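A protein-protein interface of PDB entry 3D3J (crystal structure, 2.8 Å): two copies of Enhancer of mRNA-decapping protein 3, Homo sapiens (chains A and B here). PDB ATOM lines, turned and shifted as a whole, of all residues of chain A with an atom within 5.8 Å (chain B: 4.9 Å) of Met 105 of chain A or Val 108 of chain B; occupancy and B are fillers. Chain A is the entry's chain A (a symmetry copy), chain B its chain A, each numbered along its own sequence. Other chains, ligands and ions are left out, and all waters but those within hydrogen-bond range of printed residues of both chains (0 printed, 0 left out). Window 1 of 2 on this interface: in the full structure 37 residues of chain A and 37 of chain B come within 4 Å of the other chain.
Met 105 of chain A touches just these residues of chain B: Val 108 and His 154. Gly 278 of chain A touches none of the printed residues of chain B. Of the printed residues of chain B, Phe 299 of chain A touches Ser 111 and Gln 112. Of the printed residues of chain A, Val 108 of chain B touches Met 105. Printed residues of chain A within 4 Å of Gln 112 of chain B: Gln 112 (2.9 Å) and Phe 299 (3.4 Å). Of the printed residues of chain A, His 154 of chain B touches Met 105 (3.6 Å). The nearest residue of chain B that does not touch Met 105 of chain A is Glu 104 of chain B (4.1 Å). The nearest printed residue of chain A that does not touch Glu 104 of chain B is Met 105 of chain A (4.1 Å).
SD of Met 105 of chain A touches CG2 of Val 108 of chain B (3.8 Å). His 154 of chain B touches Met 105 of chain A. SD of Met 105 of chain B touches CG2 of Val 108 of chain A, at 3.8 Å. Ser 111 of chain B touches Phe 299 of chain A (OG to CZ, 3.3 Å). CD2 of Phe 299 of chain A touches NE2 of Gln 112 of chain B, at 3.4 Å.
Met 105 of chain A touches Val 108 of chain B, and with the chains exchanged Val 108 of chain A touches Met 105 of chain B. Gln 112 of chain B touches its own counterpart, Gln 112 of chain A. Of the 7 pairs that touch across the chains among the printed residues, 3 have their exchanged pair printed and touching as well.
OE2 of Glu 104 of chain B lies within hydrogen-bond range of NE2 of His 154 of chain B (2.7 Å). The side-chain sulfur (SG) of Cys 109 of chain B lies close to the backbone carbonyl oxygen (O) of Met 105 of chain B (3.7 Å). The side-chain hydroxyl (OG) of Ser 111 of chain B lies within hydrogen-bond range of the backbone carbonyl oxygen (O) of Gly 107 of chain B (3.2 Å). The side-chain sulfur (SG) of Cys 109 of chain A sits close to the backbone carbonyl oxygen (O) of Met 105 of chain A, at 3.7 Å. N of Gly 278 of chain A sits close to SD of Met 105 of chain A (3.6 Å). N of Asp 276 of chain A is in hydrogen-bond range of O of Phe 299 of chain A (2.8 Å).
Of the 18 printed residues of chain A, 5 touch a printed residue of chain B. Hydrophobic or aromatic side chains of chain A within 4 Å of the printed part of chain B: Met 105, Val 108 and Phe 299. Of the 10 printed residues of chain B, 6 touch a printed residue of chain A. Printed residues of chain B that touch a printed residue of chain A: Glu 104, Met 105, Val 108, Ser 111, Gln 112 and His 154. Hydrophobic or aromatic side chains of chain B that line the printed part of chain A: Met 105, Val 108 and His 154. Among the printed residues, 7 pairs touch across the chains. Among the printed residues, Asp or Glu carboxylates within 4 Å of a Lys or Arg side-chain nitrogen of the other chain: Arg 101 of chain A with Glu 104 of chain B (2.8 Å).
OE1 of Glu 104 of chain B lies within salt-bridge range of NH2 of Arg 101 of chain A. OE1 of Gln 112 of chain A is in hydrogen-bond range of NE2 of Gln 112 of chain B, 2.9 Å away.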
ATOM      1  N   GLU A 100     -11.388 -10.963   2.354  1.00  0.00           N
ATOM      2  CA  GLU A 100     -11.916 -12.308   2.108  1.00  0.00           C
ATOM      3  C   GLU A 100     -11.446 -12.898   0.772  1.00  0.00           C
ATOM      4  O   GLU A 100     -11.477 -14.114   0.575  1.00  0.00           O
ATOM      5  CB  GLU A 100     -13.448 -12.366   2.263  1.00  0.00           C
ATOM      6  CG  GLU A 100     -14.266 -11.617   1.207  1.00  0.00           C
ATOM      7  CD  GLU A 100     -15.774 -11.879   1.325  1.00  0.00           C
ATOM      8  OE1 GLU A 100     -16.526 -11.542   0.378  1.00  0.00           O
ATOM      9  OE2 GLU A 100     -16.212 -12.425   2.365  1.00  0.00           O
ATOM     10  N   ARG A 101     -11.009 -12.023  -0.133  1.00  0.00           N
ATOM     11  CA  ARG A 101     -10.351 -12.446  -1.367  1.00  0.00           C
ATOM     12  C   ARG A 101      -8.931 -12.947  -1.090  1.00  0.00           C
ATOM     13  O   ARG A 101      -8.520 -13.992  -1.611  1.00  0.00           O
ATOM     14  CB  ARG A 101     -10.333 -11.314  -2.398  1.00  0.00           C
ATOM     15  CG  ARG A 101     -11.525 -11.301  -3.337  1.00  0.00           C
ATOM     16  CD  ARG A 101     -11.365 -10.218  -4.390  1.00  0.00           C
ATOM     17  NE  ARG A 101     -12.543 -10.087  -5.246  1.00  0.00           N
ATOM     18  CZ  ARG A 101     -12.634 -10.546  -6.493  1.00  0.00           C
ATOM     19  NH1 ARG A 101     -13.757 -10.363  -7.178  1.00  0.00           N
ATOM     20  NH2 ARG A 101     -11.613 -11.179  -7.064  1.00  0.00           N
ATOM     21  N   ARG A 102      -8.187 -12.202  -0.273  1.00  0.00           N
ATOM     22  CA  ARG A 102      -6.846 -12.620   0.136  1.00  0.00           C
ATOM     23  C   ARG A 102      -6.930 -13.884   0.968  1.00  0.00           C
ATOM     24  O   ARG A 102      -6.150 -14.807   0.762  1.00  0.00           O
ATOM     25  CB  ARG A 102      -6.139 -11.538   0.945  1.00  0.00           C
ATOM     26  CG  ARG A 102      -5.813 -10.263   0.184  1.00  0.00           C
ATOM     27  CD  ARG A 102      -4.638  -9.521   0.822  1.00  0.00           C
ATOM     28  NE  ARG A 102      -4.736  -9.427   2.286  1.00  0.00           N
ATOM     29  CZ  ARG A 102      -5.460  -8.525   2.952  1.00  0.00           C
ATOM     30  NH1 ARG A 102      -6.183  -7.609   2.309  1.00  0.00           N
ATOM     31  NH2 ARG A 102      -5.463  -8.542   4.277  1.00  0.00           N
ATOM     32  N   LEU A 103      -7.882 -13.922   1.896  1.00  0.00           N
ATOM     33  CA  LEU A 103      -8.083 -15.084   2.757  1.00  0.00           C
ATOM     34  C   LEU A 103      -8.396 -16.347   1.961  1.00  0.00           C
ATOM     35  O   LEU A 103      -7.878 -17.423   2.268  1.00  0.00           O
ATOM     36  CB  LEU A 103      -9.172 -14.824   3.806  1.00  0.00           C
ATOM     37  CG  LEU A 103      -8.867 -13.862   4.961  1.00  0.00           C
ATOM     38  CD1 LEU A 103      -9.982 -13.924   5.975  1.00  0.00           C
ATOM     39  CD2 LEU A 103      -7.541 -14.177   5.630  1.00  0.00           C
ATOM     40  N   GLU A 104      -9.225 -16.213   0.928  1.00  0.00           N
ATOM     41  CA  GLU A 104      -9.556 -17.354   0.096  1.00  0.00           C
ATOM     42  C   GLU A 104      -8.306 -17.862  -0.604  1.00  0.00           C
ATOM     43  O   GLU A 104      -8.013 -19.061  -0.557  1.00  0.00           O
ATOM     44  CB  GLU A 104     -10.623 -17.003  -0.930  1.00  0.00           C
ATOM     45  CG  GLU A 104     -11.257 -18.222  -1.580  1.00  0.00           C
ATOM     46  CD  GLU A 104     -11.940 -19.134  -0.577  1.00  0.00           C
ATOM     47  OE1 GLU A 104     -12.778 -18.649   0.210  1.00  0.00           O
ATOM     48  OE2 GLU A 104     -11.645 -20.337  -0.569  1.00  0.00           O
ATOM     49  N   MET A 105      -7.566 -16.942  -1.223  1.00  0.00           N
ATOM     50  CA  MET A 105      -6.377 -17.297  -2.004  1.00  0.00           C
ATOM     51  C   MET A 105      -5.253 -17.866  -1.142  1.00  0.00           C
ATOM     52  O   MET A 105      -4.666 -18.900  -1.483  1.00  0.00           O
ATOM     53  CB  MET A 105      -5.875 -16.106  -2.819  1.00  0.00           C
ATOM     54  CG  MET A 105      -4.646 -16.435  -3.643  1.00  0.00           C
ATOM     55  SD  MET A 105      -4.244 -15.181  -4.865  1.00  0.00           S
ATOM     56  CE  MET A 105      -2.803 -15.935  -5.631  1.00  0.00           C
ATOM     57  N   THR A 106      -4.961 -17.182  -0.036  1.00  0.00           N
ATOM     58  CA  THR A 106      -3.992 -17.646   0.950  1.00  0.00           C
ATOM     59  C   THR A 106      -4.371 -19.046   1.406  1.00  0.00           C
ATOM     60  O   THR A 106      -3.520 -19.918   1.504  1.00  0.00           O
ATOM     61  CB  THR A 106      -3.929 -16.678   2.160  1.00  0.00           C
ATOM     62  OG1 THR A 106      -3.590 -15.362   1.702  1.00  0.00           O
ATOM     63  CG2 THR A 106      -2.907 -17.130   3.199  1.00  0.00           C
ATOM     64  N   GLY A 107      -5.660 -19.254   1.658  1.00  0.00           N
ATOM     65  CA  GLY A 107      -6.179 -20.562   2.044  1.00  0.00           C
ATOM     66  C   GLY A 107      -5.767 -21.623   1.049  1.00  0.00           C
ATOM     67  O   GLY A 107      -5.118 -22.603   1.423  1.00  0.00           O
ATOM     68  N   VAL A 108      -6.130 -21.402  -0.217  1.00  0.00           N
ATOM     69  CA  VAL A 108      -5.840 -22.321  -1.325  1.00  0.00           C
ATOM     70  C   VAL A 108      -4.344 -22.616  -1.457  1.00  0.00           C
ATOM     71  O   VAL A 108      -3.914 -23.775  -1.420  1.00  0.00           O
ATOM     72  CB  VAL A 108      -6.393 -21.769  -2.683  1.00  0.00           C
ATOM     73  CG1 VAL A 108      -5.726 -22.435  -3.882  1.00  0.00           C
ATOM     74  CG2 VAL A 108      -7.890 -21.948  -2.760  1.00  0.00           C
ATOM     75  N   CYS A 109      -3.559 -21.556  -1.601  1.00  0.00           N
ATOM     76  CA  CYS A 109      -2.139 -21.689  -1.857  1.00  0.00           C
ATOM     77  C   CYS A 109      -1.390 -22.306  -0.685  1.00  0.00           C
ATOM     78  O   CYS A 109      -0.500 -23.139  -0.887  1.00  0.00           O
ATOM     79  CB  CYS A 109      -1.565 -20.338  -2.264  1.00  0.00           C
ATOM     80  SG  CYS A 109      -2.131 -19.860  -3.928  1.00  0.00           S
ATOM     81  N   ALA A 110      -1.762 -21.921   0.538  1.00  0.00           N
ATOM     82  CA  ALA A 110      -1.178 -22.521   1.734  1.00  0.00           C
ATOM     83  C   ALA A 110      -1.524 -24.008   1.832  1.00  0.00           C
ATOM     84  O   ALA A 110      -0.687 -24.830   2.229  1.00  0.00           O
ATOM     85  CB  ALA A 110      -1.625 -21.780   2.985  1.00  0.00           C
ATOM     86  N   GLN A 112      -2.247 -25.950  -0.651  1.00  0.00           N
ATOM     87  CA  GLN A 112      -1.491 -26.568  -1.745  1.00  0.00           C
ATOM     88  C   GLN A 112      -0.049 -26.881  -1.352  1.00  0.00           C
ATOM     89  O   GLN A 112       0.501 -27.919  -1.745  1.00  0.00           O
ATOM     90  CB  GLN A 112      -1.533 -25.688  -2.993  1.00  0.00           C
ATOM     91  CG  GLN A 112      -2.791 -25.872  -3.822  1.00  0.00           C
ATOM     92  CD  GLN A 112      -2.896 -24.909  -4.990  1.00  0.00           C
ATOM     93  OE1 GLN A 112      -2.068 -24.016  -5.162  1.00  0.00           O
ATOM     94  NE2 GLN A 112      -3.925 -25.088  -5.802  1.00  0.00           N
ATOM     95  N   SER A 150      -8.752 -20.725   6.952  1.00  0.00           N
ATOM     96  CA  SER A 150      -9.004 -20.819   5.518  1.00  0.00           C
ATOM     97  C   SER A 150      -8.199 -21.965   4.926  1.00  0.00           C
ATOM     98  O   SER A 150      -8.715 -22.765   4.150  1.00  0.00           O
ATOM     99  CB  SER A 150      -8.640 -19.504   4.827  1.00  0.00           C
ATOM    100  OG  SER A 150      -8.902 -19.560   3.437  1.00  0.00           O
ATOM    101  N   CYS A 275       4.646 -17.196  -0.873  1.00  0.00           N
ATOM    102  CA  CYS A 275       3.370 -17.455  -1.468  1.00  0.00           C
ATOM    103  C   CYS A 275       2.890 -16.226  -2.233  1.00  0.00           C
ATOM    104  O   CYS A 275       3.168 -15.085  -1.852  1.00  0.00           O
ATOM    105  CB  CYS A 275       2.398 -17.775  -0.349  1.00  0.00           C
ATOM    106  SG  CYS A 275       0.752 -18.017  -0.900  1.00  0.00           S
ATOM    107  N   ASP A 276       2.157 -16.470  -3.313  1.00  0.00           N
ATOM    108  CA  ASP A 276       1.542 -15.401  -4.097  1.00  0.00           C
ATOM    109  C   ASP A 276       0.146 -15.105  -3.547  1.00  0.00           C
ATOM    110  O   ASP A 276      -0.674 -16.010  -3.423  1.00  0.00           O
ATOM    111  CB  ASP A 276       1.471 -15.831  -5.567  1.00  0.00           C
ATOM    112  CG  ASP A 276       0.749 -14.826  -6.453  1.00  0.00           C
ATOM    113  OD1 ASP A 276       0.798 -13.612  -6.167  1.00  0.00           O
ATOM    114  OD2 ASP A 276       0.142 -15.258  -7.459  1.00  0.00           O
ATOM    115  N   ILE A 277      -0.118 -13.849  -3.193  1.00  0.00           N
ATOM    116  CA  ILE A 277      -1.473 -13.455  -2.766  1.00  0.00           C
ATOM    117  C   ILE A 277      -2.188 -12.564  -3.786  1.00  0.00           C
ATOM    118  O   ILE A 277      -3.164 -11.883  -3.461  1.00  0.00           O
ATOM    119  CB  ILE A 277      -1.529 -12.851  -1.334  1.00  0.00           C
ATOM    120  CG1 ILE A 277      -0.340 -11.920  -1.090  1.00  0.00           C
ATOM    121  CG2 ILE A 277      -1.591 -13.964  -0.288  1.00  0.00           C
ATOM    122  CD1 ILE A 277      -0.461 -11.078   0.154  1.00  0.00           C
ATOM    123  N   GLY A 278      -1.703 -12.602  -5.024  1.00  0.00           N
ATOM    124  CA  GLY A 278      -2.367 -11.962  -6.147  1.00  0.00           C
ATOM    125  C   GLY A 278      -2.359 -10.449  -6.078  1.00  0.00           C
ATOM    126  O   GLY A 278      -3.357  -9.800  -6.407  1.00  0.00           O
ATOM    127  N   PHE A 299       2.777 -20.767  -7.537  1.00  0.00           N
ATOM    128  CA  PHE A 299       2.146 -19.874  -6.568  1.00  0.00           C
ATOM    129  C   PHE A 299       2.830 -19.919  -5.194  1.00  0.00           C
ATOM    130  O   PHE A 299       2.622 -19.031  -4.360  1.00  0.00           O
ATOM    131  CB  PHE A 299       0.649 -20.180  -6.449  1.00  0.00           C
ATOM    132  CG  PHE A 299      -0.176 -19.621  -7.576  1.00  0.00           C
ATOM    133  CD1 PHE A 299      -1.060 -18.568  -7.346  1.00  0.00           C
ATOM    134  CD2 PHE A 299      -0.072 -20.142  -8.869  1.00  0.00           C
ATOM    135  CE1 PHE A 299      -1.828 -18.045  -8.385  1.00  0.00           C
ATOM    136  CE2 PHE A 299      -0.827 -19.626  -9.910  1.00  0.00           C
ATOM    137  CZ  PHE A 299      -1.713 -18.572  -9.668  1.00  0.00           C
ATOM    138  N   GLU B 104     -12.299 -15.517  -6.911  1.00  0.00           N
ATOM    139  CA  GLU B 104     -10.883 -15.498  -6.604  1.00  0.00           C
ATOM    140  C   GLU B 104     -10.295 -16.885  -6.794  1.00  0.00           C
ATOM    141  O   GLU B 104      -9.275 -17.039  -7.475  1.00  0.00           O
ATOM    142  CB  GLU B 104     -10.628 -15.010  -5.186  1.00  0.00           C
ATOM    143  CG  GLU B 104      -9.176 -14.633  -4.930  1.00  0.00           C
ATOM    144  CD  GLU B 104      -8.693 -13.517  -5.837  1.00  0.00           C
ATOM    145  OE1 GLU B 104      -9.350 -12.459  -5.900  1.00  0.00           O
ATOM    146  OE2 GLU B 104      -7.654 -13.690  -6.491  1.00  0.00           O
ATOM    147  N   MET B 105     -10.956 -17.887  -6.213  1.00  0.00           N
ATOM    148  CA  MET B 105     -10.462 -19.266  -6.246  1.00  0.00           C
ATOM    149  C   MET B 105     -10.460 -19.859  -7.652  1.00  0.00           C
ATOM    150  O   MET B 105      -9.465 -20.457  -8.077  1.00  0.00           O
ATOM    151  CB  MET B 105     -11.253 -20.159  -5.291  1.00  0.00           C
ATOM    152  CG  MET B 105     -10.770 -21.596  -5.296  1.00  0.00           C
ATOM    153  SD  MET B 105     -11.433 -22.581  -3.947  1.00  0.00           S
ATOM    154  CE  MET B 105     -10.620 -24.151  -4.272  1.00  0.00           C
ATOM    155  N   THR B 106     -11.578 -19.692  -8.359  1.00  0.00           N
ATOM    156  CA  THR B 106     -11.703 -20.100  -9.753  1.00  0.00           C
ATOM    157  C   THR B 106     -10.588 -19.457 -10.566  1.00  0.00           C
ATOM    158  O   THR B 106      -9.958 -20.114 -11.381  1.00  0.00           O
ATOM    159  CB  THR B 106     -13.089 -19.701 -10.323  1.00  0.00           C
ATOM    160  OG1 THR B 106     -14.120 -20.303  -9.530  1.00  0.00           O
ATOM    161  CG2 THR B 106     -13.253 -20.133 -11.778  1.00  0.00           C
ATOM    162  N   GLY B 107     -10.340 -18.175 -10.314  1.00  0.00           N
ATOM    163  CA  GLY B 107      -9.261 -17.445 -10.970  1.00  0.00           C
ATOM    164  C   GLY B 107      -7.943 -18.167 -10.813  1.00  0.00           C
ATOM    165  O   GLY B 107      -7.305 -18.514 -11.809  1.00  0.00           O
ATOM    166  N   VAL B 108      -7.561 -18.408  -9.557  1.00  0.00           N
ATOM    167  CA  VAL B 108      -6.307 -19.082  -9.196  1.00  0.00           C
ATOM    168  C   VAL B 108      -6.181 -20.460  -9.848  1.00  0.00           C
ATOM    169  O   VAL B 108      -5.212 -20.743 -10.563  1.00  0.00           O
ATOM    170  CB  VAL B 108      -6.159 -19.215  -7.641  1.00  0.00           C
ATOM    171  CG1 VAL B 108      -5.144 -20.286  -7.257  1.00  0.00           C
ATOM    172  CG2 VAL B 108      -5.772 -17.892  -7.027  1.00  0.00           C
ATOM    173  N   CYS B 109      -7.174 -21.305  -9.603  1.00  0.00           N
ATOM    174  CA  CYS B 109      -7.132 -22.682 -10.055  1.00  0.00           C
ATOM    175  C   CYS B 109      -7.168 -22.799 -11.574  1.00  0.00           C
ATOM    176  O   CYS B 109      -6.450 -23.625 -12.149  1.00  0.00           O
ATOM    177  CB  CYS B 109      -8.247 -23.473  -9.386  1.00  0.00           C
ATOM    178  SG  CYS B 109      -7.901 -23.725  -7.616  1.00  0.00           S
ATOM    179  N   ALA B 110      -7.980 -21.963 -12.222  1.00  0.00           N
ATOM    180  CA  ALA B 110      -8.022 -21.923 -13.680  1.00  0.00           C
ATOM    181  C   ALA B 110      -6.682 -21.459 -14.260  1.00  0.00           C
ATOM    182  O   ALA B 110      -6.220 -21.978 -15.285  1.00  0.00           O
ATOM    183  CB  ALA B 110      -9.155 -21.034 -14.166  1.00  0.00           C
ATOM    184  N   SER B 111      -6.058 -20.490 -13.595  1.00  0.00           N
ATOM    185  CA  SER B 111      -4.795 -19.949 -14.073  1.00  0.00           C
ATOM    186  C   SER B 111      -3.719 -21.002 -13.923  1.00  0.00           C
ATOM    187  O   SER B 111      -2.859 -21.146 -14.792  1.00  0.00           O
ATOM    188  CB  SER B 111      -4.417 -18.669 -13.326  1.00  0.00           C
ATOM    189  OG  SER B 111      -4.111 -18.932 -11.971  1.00  0.00           O
ATOM    190  N   GLN B 112      -3.800 -21.746 -12.822  1.00  0.00           N
ATOM    191  CA  GLN B 112      -2.882 -22.853 -12.538  1.00  0.00           C
ATOM    192  C   GLN B 112      -2.955 -23.954 -13.595  1.00  0.00           C
ATOM    193  O   GLN B 112      -1.928 -24.542 -13.963  1.00  0.00           O
ATOM    194  CB  GLN B 112      -3.142 -23.423 -11.143  1.00  0.00           C
ATOM    195  CG  GLN B 112      -2.464 -22.640 -10.035  1.00  0.00           C
ATOM    196  CD  GLN B 112      -2.822 -23.126  -8.641  1.00  0.00           C
ATOM    197  OE1 GLN B 112      -3.659 -24.009  -8.465  1.00  0.00           O
ATOM    198  NE2 GLN B 112      -2.187 -22.541  -7.640  1.00  0.00           N
ATOM    199  N   HIS B 154      -4.740 -13.393 -12.831  1.00  0.00           N
ATOM    200  CA  HIS B 154      -3.754 -14.250 -12.181  1.00  0.00           C
ATOM    201  C   HIS B 154      -2.612 -14.627 -13.109  1.00  0.00           C
ATOM    202  O   HIS B 154      -1.453 -14.643 -12.699  1.00  0.00           O
ATOM    203  CB  HIS B 154      -4.421 -15.486 -11.588  1.00  0.00           C
ATOM    204  CG  HIS B 154      -5.167 -15.201 -10.323  1.00  0.00           C
ATOM    205  ND1 HIS B 154      -4.531 -14.832  -9.155  1.00  0.00           N
ATOM    206  CD2 HIS B 154      -6.492 -15.210 -10.046  1.00  0.00           C
ATOM    207  CE1 HIS B 154      -5.434 -14.636  -8.211  1.00  0.00           C
ATOM    208  NE2 HIS B 154      -6.631 -14.858  -8.725  1.00  0.00           N
